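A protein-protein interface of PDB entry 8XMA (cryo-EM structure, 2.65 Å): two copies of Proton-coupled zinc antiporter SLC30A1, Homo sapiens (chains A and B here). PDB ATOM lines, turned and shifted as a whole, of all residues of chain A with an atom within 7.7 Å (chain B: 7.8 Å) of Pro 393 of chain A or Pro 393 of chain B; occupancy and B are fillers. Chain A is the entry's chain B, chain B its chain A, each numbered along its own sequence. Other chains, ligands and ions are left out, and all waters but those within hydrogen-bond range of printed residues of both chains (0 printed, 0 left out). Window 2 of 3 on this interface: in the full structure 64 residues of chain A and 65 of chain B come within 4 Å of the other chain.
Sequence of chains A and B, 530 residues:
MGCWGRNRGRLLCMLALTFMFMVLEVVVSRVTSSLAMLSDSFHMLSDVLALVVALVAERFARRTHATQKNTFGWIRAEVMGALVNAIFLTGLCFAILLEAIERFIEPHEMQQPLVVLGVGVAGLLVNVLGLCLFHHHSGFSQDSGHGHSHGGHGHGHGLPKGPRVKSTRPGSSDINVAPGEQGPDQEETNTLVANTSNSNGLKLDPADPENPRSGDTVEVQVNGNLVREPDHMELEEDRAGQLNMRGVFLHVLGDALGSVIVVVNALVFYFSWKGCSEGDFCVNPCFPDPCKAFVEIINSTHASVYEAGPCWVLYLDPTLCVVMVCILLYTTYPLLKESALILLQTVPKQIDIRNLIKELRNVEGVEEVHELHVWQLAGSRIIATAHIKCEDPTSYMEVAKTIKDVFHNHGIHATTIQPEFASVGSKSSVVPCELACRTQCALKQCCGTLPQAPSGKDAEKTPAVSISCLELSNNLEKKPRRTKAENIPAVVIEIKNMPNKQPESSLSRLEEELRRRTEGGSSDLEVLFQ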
ATOM      1  N   CYS A 390      -8.801   7.414  25.962  1.00  0.00           N
ATOM      2  CA  CYS A 390      -9.487   8.539  25.338  1.00  0.00           C
ATOM      3  C   CYS A 390     -10.338   8.149  24.142  1.00  0.00           C
ATOM      4  O   CYS A 390     -11.390   8.755  23.921  1.00  0.00           O
ATOM      5  CB  CYS A 390      -8.469   9.598  24.903  1.00  0.00           C
ATOM      6  SG  CYS A 390      -7.585  10.383  26.266  1.00  0.00           S
ATOM      7  N   GLU A 391      -9.901   7.161  23.359  1.00  0.00           N
ATOM      8  CA  GLU A 391     -10.605   6.715  22.155  1.00  0.00           C
ATOM      9  C   GLU A 391     -10.773   7.848  21.144  1.00  0.00           C
ATOM     10  O   GLU A 391     -11.701   7.837  20.332  1.00  0.00           O
ATOM     11  CB  GLU A 391     -11.965   6.098  22.499  1.00  0.00           C
ATOM     12  N   ASP A 392      -9.872   8.830  21.184  1.00  0.00           N
ATOM     13  CA  ASP A 392      -9.905   9.965  20.271  1.00  0.00           C
ATOM     14  C   ASP A 392      -8.539  10.638  20.237  1.00  0.00           C
ATOM     15  O   ASP A 392      -8.338  11.667  20.895  1.00  0.00           O
ATOM     16  CB  ASP A 392     -10.985  10.965  20.687  1.00  0.00           C
ATOM     17  N   PRO A 393      -7.577  10.088  19.492  1.00  0.00           N
ATOM     18  CA  PRO A 393      -6.236  10.693  19.459  1.00  0.00           C
ATOM     19  C   PRO A 393      -6.210  12.103  18.896  1.00  0.00           C
ATOM     20  O   PRO A 393      -5.301  12.871  19.237  1.00  0.00           O
ATOM     21  CB  PRO A 393      -5.436   9.725  18.576  1.00  0.00           C
ATOM     22  CG  PRO A 393      -6.467   9.027  17.750  1.00  0.00           C
ATOM     23  CD  PRO A 393      -7.670   8.896  18.633  1.00  0.00           C
ATOM     24  N   THR A 394      -7.172  12.472  18.048  1.00  0.00           N
ATOM     25  CA  THR A 394      -7.188  13.801  17.453  1.00  0.00           C
ATOM     26  C   THR A 394      -7.391  14.906  18.483  1.00  0.00           C
ATOM     27  O   THR A 394      -6.741  15.953  18.386  1.00  0.00           O
ATOM     28  CB  THR A 394      -8.283  13.887  16.386  1.00  0.00           C
ATOM     29  OG1 THR A 394      -8.088  12.847  15.418  1.00  0.00           O
ATOM     30  CG2 THR A 394      -8.243  15.235  15.682  1.00  0.00           C
ATOM     31  N   SER A 395      -8.263  14.695  19.465  1.00  0.00           N
ATOM     32  CA  SER A 395      -8.548  15.692  20.487  1.00  0.00           C
ATOM     33  C   SER A 395      -7.788  15.450  21.784  1.00  0.00           C
ATOM     34  O   SER A 395      -8.239  15.902  22.840  1.00  0.00           O
ATOM     35  CB  SER A 395     -10.052  15.738  20.774  1.00  0.00           C
ATOM     36  N   TYR A 396      -6.654  14.747  21.732  1.00  0.00           N
ATOM     37  CA  TYR A 396      -5.897  14.453  22.944  1.00  0.00           C
ATOM     38  C   TYR A 396      -5.414  15.722  23.635  1.00  0.00           C
ATOM     39  O   TYR A 396      -5.509  15.851  24.860  1.00  0.00           O
ATOM     40  CB  TYR A 396      -4.711  13.543  22.612  1.00  0.00           C
ATOM     41  CG  TYR A 396      -3.729  13.396  23.754  1.00  0.00           C
ATOM     42  CD1 TYR A 396      -4.164  13.068  25.032  1.00  0.00           C
ATOM     43  CD2 TYR A 396      -2.371  13.597  23.556  1.00  0.00           C
ATOM     44  CE1 TYR A 396      -3.273  12.943  26.076  1.00  0.00           C
ATOM     45  CE2 TYR A 396      -1.473  13.470  24.596  1.00  0.00           C
ATOM     46  CZ  TYR A 396      -1.929  13.144  25.854  1.00  0.00           C
ATOM     47  OH  TYR A 396      -1.037  13.016  26.893  1.00  0.00           O
ATOM     48  N   MET A 397      -4.889  16.676  22.862  1.00  0.00           N
ATOM     49  CA  MET A 397      -4.391  17.909  23.464  1.00  0.00           C
ATOM     50  C   MET A 397      -5.502  18.698  24.141  1.00  0.00           C
ATOM     51  O   MET A 397      -5.238  19.463  25.076  1.00  0.00           O
ATOM     52  CB  MET A 397      -3.690  18.765  22.410  1.00  0.00           C
ATOM     53  CG  MET A 397      -2.352  18.203  21.972  1.00  0.00           C
ATOM     54  SD  MET A 397      -1.502  17.422  23.357  1.00  0.00           S
ATOM     55  CE  MET A 397       0.138  17.213  22.678  1.00  0.00           C
ATOM     56  N   GLU A 398      -6.746  18.529  23.689  1.00  0.00           N
ATOM     57  CA  GLU A 398      -7.866  19.165  24.373  1.00  0.00           C
ATOM     58  C   GLU A 398      -8.043  18.602  25.778  1.00  0.00           C
ATOM     59  O   GLU A 398      -8.333  19.349  26.719  1.00  0.00           O
ATOM     60  CB  GLU A 398      -9.147  18.992  23.557  1.00  0.00           C
ATOM     61  N   PRO A 419      -1.741   8.116  27.413  1.00  0.00           N
ATOM     62  CA  PRO A 419      -3.023   7.718  26.829  1.00  0.00           C
ATOM     63  C   PRO A 419      -2.970   6.304  26.277  1.00  0.00           C
ATOM     64  O   PRO A 419      -1.907   5.786  25.927  1.00  0.00           O
ATOM     65  CB  PRO A 419      -3.238   8.737  25.701  1.00  0.00           C
ATOM     66  CG  PRO A 419      -2.139   9.743  25.838  1.00  0.00           C
ATOM     67  CD  PRO A 419      -1.030   9.082  26.569  1.00  0.00           C
ATOM     68  N   GLU A 420      -4.141   5.679  26.204  1.00  0.00           N
ATOM     69  CA  GLU A 420      -4.309   4.386  25.557  1.00  0.00           C
ATOM     70  C   GLU A 420      -5.555   4.439  24.687  1.00  0.00           C
ATOM     71  O   GLU A 420      -6.597   4.936  25.123  1.00  0.00           O
ATOM     72  CB  GLU A 420      -4.417   3.252  26.582  1.00  0.00           C
ATOM     73  CG  GLU A 420      -3.275   3.205  27.585  1.00  0.00           C
ATOM     74  CD  GLU A 420      -3.516   2.211  28.699  1.00  0.00           C
ATOM     75  OE1 GLU A 420      -4.408   1.351  28.548  1.00  0.00           O
ATOM     76  OE2 GLU A 420      -2.812   2.285  29.727  1.00  0.00           O
ATOM     77  N   PHE A 421      -5.446   3.933  23.463  1.00  0.00           N
ATOM     78  CA  PHE A 421      -6.542   3.954  22.507  1.00  0.00           C
ATOM     79  C   PHE A 421      -6.848   2.538  22.042  1.00  0.00           C
ATOM     80  O   PHE A 421      -5.938   1.726  21.852  1.00  0.00           O
ATOM     81  CB  PHE A 421      -6.209   4.840  21.302  1.00  0.00           C
ATOM     82  CG  PHE A 421      -5.741   6.217  21.676  1.00  0.00           C
ATOM     83  CD1 PHE A 421      -6.653   7.227  21.928  1.00  0.00           C
ATOM     84  CD2 PHE A 421      -4.391   6.503  21.771  1.00  0.00           C
ATOM     85  CE1 PHE A 421      -6.225   8.494  22.272  1.00  0.00           C
ATOM     86  CE2 PHE A 421      -3.959   7.769  22.112  1.00  0.00           C
ATOM     87  CZ  PHE A 421      -4.877   8.766  22.363  1.00  0.00           C
ATOM     88  N   ALA A 422      -8.132   2.249  21.859  1.00  0.00           N
ATOM     89  CA  ALA A 422      -8.561   0.928  21.418  1.00  0.00           C
ATOM     90  C   ALA A 422      -8.552   0.831  19.896  1.00  0.00           C
ATOM     91  O   ALA A 422      -8.904   1.784  19.201  1.00  0.00           O
ATOM     92  CB  ALA A 422      -9.944   0.611  21.962  1.00  0.00           C
ATOM     93  N   CYS B 390       5.751  12.853  18.970  1.00  0.00           N
ATOM     94  CA  CYS B 390       5.454  12.046  17.798  1.00  0.00           C
ATOM     95  C   CYS B 390       5.157  12.937  16.596  1.00  0.00           C
ATOM     96  O   CYS B 390       4.862  14.127  16.723  1.00  0.00           O
ATOM     97  CB  CYS B 390       4.275  11.109  18.075  1.00  0.00           C
ATOM     98  SG  CYS B 390       4.599   9.860  19.338  1.00  0.00           S
ATOM     99  N   GLU B 391       5.250  12.334  15.409  1.00  0.00           N
ATOM    100  CA  GLU B 391       4.971  13.071  14.180  1.00  0.00           C
ATOM    101  C   GLU B 391       3.503  13.470  14.098  1.00  0.00           C
ATOM    102  O   GLU B 391       3.178  14.608  13.738  1.00  0.00           O
ATOM    103  CB  GLU B 391       5.371  12.231  12.966  1.00  0.00           C
ATOM    104  N   ASP B 392       2.599  12.546  14.430  1.00  0.00           N
ATOM    105  CA  ASP B 392       1.171  12.804  14.368  1.00  0.00           C
ATOM    106  C   ASP B 392       0.454  11.859  15.320  1.00  0.00           C
ATOM    107  O   ASP B 392       0.934  10.738  15.543  1.00  0.00           O
ATOM    108  CB  ASP B 392       0.626  12.624  12.947  1.00  0.00           C
ATOM    109  N   PRO B 393      -0.678  12.273  15.893  1.00  0.00           N
ATOM    110  CA  PRO B 393      -1.435  11.357  16.763  1.00  0.00           C
ATOM    111  C   PRO B 393      -1.920  10.110  16.047  1.00  0.00           C
ATOM    112  O   PRO B 393      -2.116   9.071  16.690  1.00  0.00           O
ATOM    113  CB  PRO B 393      -2.605  12.224  17.248  1.00  0.00           C
ATOM    114  CG  PRO B 393      -2.727  13.310  16.231  1.00  0.00           C
ATOM    115  CD  PRO B 393      -1.328  13.588  15.775  1.00  0.00           C
ATOM    116  N   THR B 394      -2.133  10.183  14.735  1.00  0.00           N
ATOM    117  CA  THR B 394      -2.509   9.002  13.973  1.00  0.00           C
ATOM    118  C   THR B 394      -1.364   7.996  13.968  1.00  0.00           C
ATOM    119  O   THR B 394      -0.196   8.364  13.811  1.00  0.00           O
ATOM    120  CB  THR B 394      -2.882   9.389  12.542  1.00  0.00           C
ATOM    121  OG1 THR B 394      -3.929  10.367  12.568  1.00  0.00           O
ATOM    122  CG2 THR B 394      -3.357   8.172  11.761  1.00  0.00           C
ATOM    123  N   SER B 395      -1.708   6.720  14.155  1.00  0.00           N
ATOM    124  CA  SER B 395      -0.735   5.629  14.221  1.00  0.00           C
ATOM    125  C   SER B 395       0.272   5.834  15.350  1.00  0.00           C
ATOM    126  O   SER B 395       1.413   5.373  15.271  1.00  0.00           O
ATOM    127  CB  SER B 395      -0.010   5.445  12.884  1.00  0.00           C
ATOM    128  N   TYR B 396      -0.145   6.532  16.408  1.00  0.00           N
ATOM    129  CA  TYR B 396       0.718   6.697  17.572  1.00  0.00           C
ATOM    130  C   TYR B 396       0.902   5.380  18.315  1.00  0.00           C
ATOM    131  O   TYR B 396       1.977   5.115  18.862  1.00  0.00           O
ATOM    132  CB  TYR B 396       0.143   7.757  18.512  1.00  0.00           C
ATOM    133  CG  TYR B 396       0.512   7.547  19.963  1.00  0.00           C
ATOM    134  CD1 TYR B 396       1.806   7.777  20.412  1.00  0.00           C
ATOM    135  CD2 TYR B 396      -0.428   7.101  20.881  1.00  0.00           C
ATOM    136  CE1 TYR B 396       2.148   7.576  21.734  1.00  0.00           C
ATOM    137  CE2 TYR B 396      -0.094   6.898  22.204  1.00  0.00           C
ATOM    138  CZ  TYR B 396       1.194   7.136  22.625  1.00  0.00           C
ATOM    139  OH  TYR B 396       1.532   6.937  23.944  1.00  0.00           O
ATOM    140  N   MET B 397      -0.138   4.542  18.341  1.00  0.00           N
ATOM    141  CA  MET B 397      -0.102   3.345  19.173  1.00  0.00           C
ATOM    142  C   MET B 397       1.009   2.396  18.747  1.00  0.00           C
ATOM    143  O   MET B 397       1.532   1.642  19.576  1.00  0.00           O
ATOM    144  CB  MET B 397      -1.456   2.638  19.127  1.00  0.00           C
ATOM    145  CG  MET B 397      -1.741   1.791  20.350  1.00  0.00           C
ATOM    146  SD  MET B 397      -2.102   2.840  21.772  1.00  0.00           S
ATOM    147  CE  MET B 397      -1.861   1.694  23.123  1.00  0.00           C
ATOM    148  N   GLU B 398       1.382   2.416  17.465  1.00  0.00           N
ATOM    149  CA  GLU B 398       2.525   1.627  17.012  1.00  0.00           C
ATOM    150  C   GLU B 398       3.813   2.109  17.668  1.00  0.00           C
ATOM    151  O   GLU B 398       4.670   1.302  18.045  1.00  0.00           O
ATOM    152  CB  GLU B 398       2.635   1.691  15.489  1.00  0.00           C
ATOM    153  N   PRO B 419       3.088  11.015  25.137  1.00  0.00           N
ATOM    154  CA  PRO B 419       3.359  11.687  23.865  1.00  0.00           C
ATOM    155  C   PRO B 419       3.018  13.165  23.929  1.00  0.00           C
ATOM    156  O   PRO B 419       2.116  13.591  24.654  1.00  0.00           O
ATOM    157  CB  PRO B 419       2.453  10.951  22.875  1.00  0.00           C
ATOM    158  CG  PRO B 419       1.344  10.428  23.713  1.00  0.00           C
ATOM    159  CD  PRO B 419       1.958  10.078  25.035  1.00  0.00           C
ATOM    160  N   PHE B 421       2.388  15.718  20.920  1.00  0.00           N
ATOM    161  CA  PHE B 421       2.273  16.025  19.505  1.00  0.00           C
ATOM    162  C   PHE B 421       2.409  17.525  19.263  1.00  0.00           C
ATOM    163  O   PHE B 421       2.240  18.348  20.167  1.00  0.00           O
ATOM    164  CB  PHE B 421       0.938  15.525  18.956  1.00  0.00           C
ATOM    165  CG  PHE B 421       0.583  14.138  19.401  1.00  0.00           C
ATOM    166  CD1 PHE B 421       1.386  13.063  19.065  1.00  0.00           C
ATOM    167  CD2 PHE B 421      -0.551  13.909  20.158  1.00  0.00           C
ATOM    168  CE1 PHE B 421       1.063  11.784  19.475  1.00  0.00           C
ATOM    169  CE2 PHE B 421      -0.879  12.633  20.570  1.00  0.00           C
ATOM    170  CZ  PHE B 421      -0.071  11.570  20.228  1.00  0.00           C
ATOM    171  N   ALA B 422       2.722  17.872  18.020  1.00  0.00           N
ATOM    172  CA  ALA B 422       2.892  19.267  17.632  1.00  0.00           C
ATOM    173  C   ALA B 422       1.570  19.871  17.172  1.00  0.00           C
ATOM    174  O   ALA B 422       1.337  21.070  17.328  1.00  0.00           O
ATOM    175  CB  ALA B 422       3.940  19.387  16.538  1.00  0.00           C
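Pro 393 of chain A touches its own counterpart, Pro 393 of chain B.
Tyr 396 of chain A touches Pro 419 of chain B, but with the chains exchanged Pro 419 of chain A does not touch Tyr 396 of chain B (4.1 Å).
Tyr 396 of chain A touches Phe 421 of chain B, and with the chains exchanged Phe 421 of chain A touches Tyr 396 of chain B.
Met 397 of chain A touches Phe 421 of chain B, and with the chains exchanged Phe 421 of chain A touches Met 397 of chain B.
Of the 7 pairs that touch across the chains among the printed residues, 6 have their exchanged pair printed and touching as well.
No residue of chain B comes within 4 Å of Asp 392 of chain A.
Pro 393 of chain A touches just one residue of chain B: Pro 393.
Printed residues of chain B within 4 Å of Tyr 396 of chain A: Pro 419 and Phe 421.
Printed residues of chain B within 4 Å of Pro 419 of chain A: Pro 419 (3.5 Å).
Ala 422 of chain A touches none of the printed residues of chain B.
Cys 390 of chain B touches none of the printed residues of chain A.
No residue of chain A comes within 4 Å of Asp 392 of chain B.
Pro 393 of chain B touches one residue of chain A.
Printed residues of chain A within 4 Å of Tyr 396 of chain B: Phe 421.
Of the printed residues of chain A, Pro 419 of chain B touches Tyr 396 (3.6 Å) and Pro 419 (3.5 Å).
The nearest residue of chain A that does not touch Pro 393 of chain B is Thr 394 of chain A (4.6 Å).
Among the printed residues, pairs that only touch across the chains: Pro 393 of chain A with Pro 393 of chain B (3.4 Å), Tyr 396 of chain A with Pro 419 of chain B (3.6 Å), Tyr 396 of chain A with Phe 421 of chain B (3.5 Å), Met 397 of chain A with Phe 421 of chain B (3.2 Å), Pro 419 of chain A with Pro 419 of chain B (3.5 Å), Phe 421 of chain A with Tyr 396 of chain B (3.8 Å) and Phe 421 of chain A with Met 397 of chain B (3.9 Å).
Of the 13 printed residues of chain A, 5 touch a printed residue of chain B.
Printed residues of chain A that touch a printed residue of chain B: Pro 393, Tyr 396, Met 397, Pro 419 and Phe 421.
Hydrophobic or aromatic side chains of chain A within 4 Å of the printed part of chain B: Pro 393, Tyr 396, Met 397, Pro 419 and Phe 421.
Along chain A the printed residues that touch a printed residue of chain B span positions 393 to 421.
Along chain B the printed residues that touch a printed residue of chain A span positions 393 to 421.
Among the printed residues, 7 pairs touch across the chains.
Among the printed residues, no Asp or Glu carboxylate lies within 4 Å of a Lys or Arg side-chain nitrogen of the other chain.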
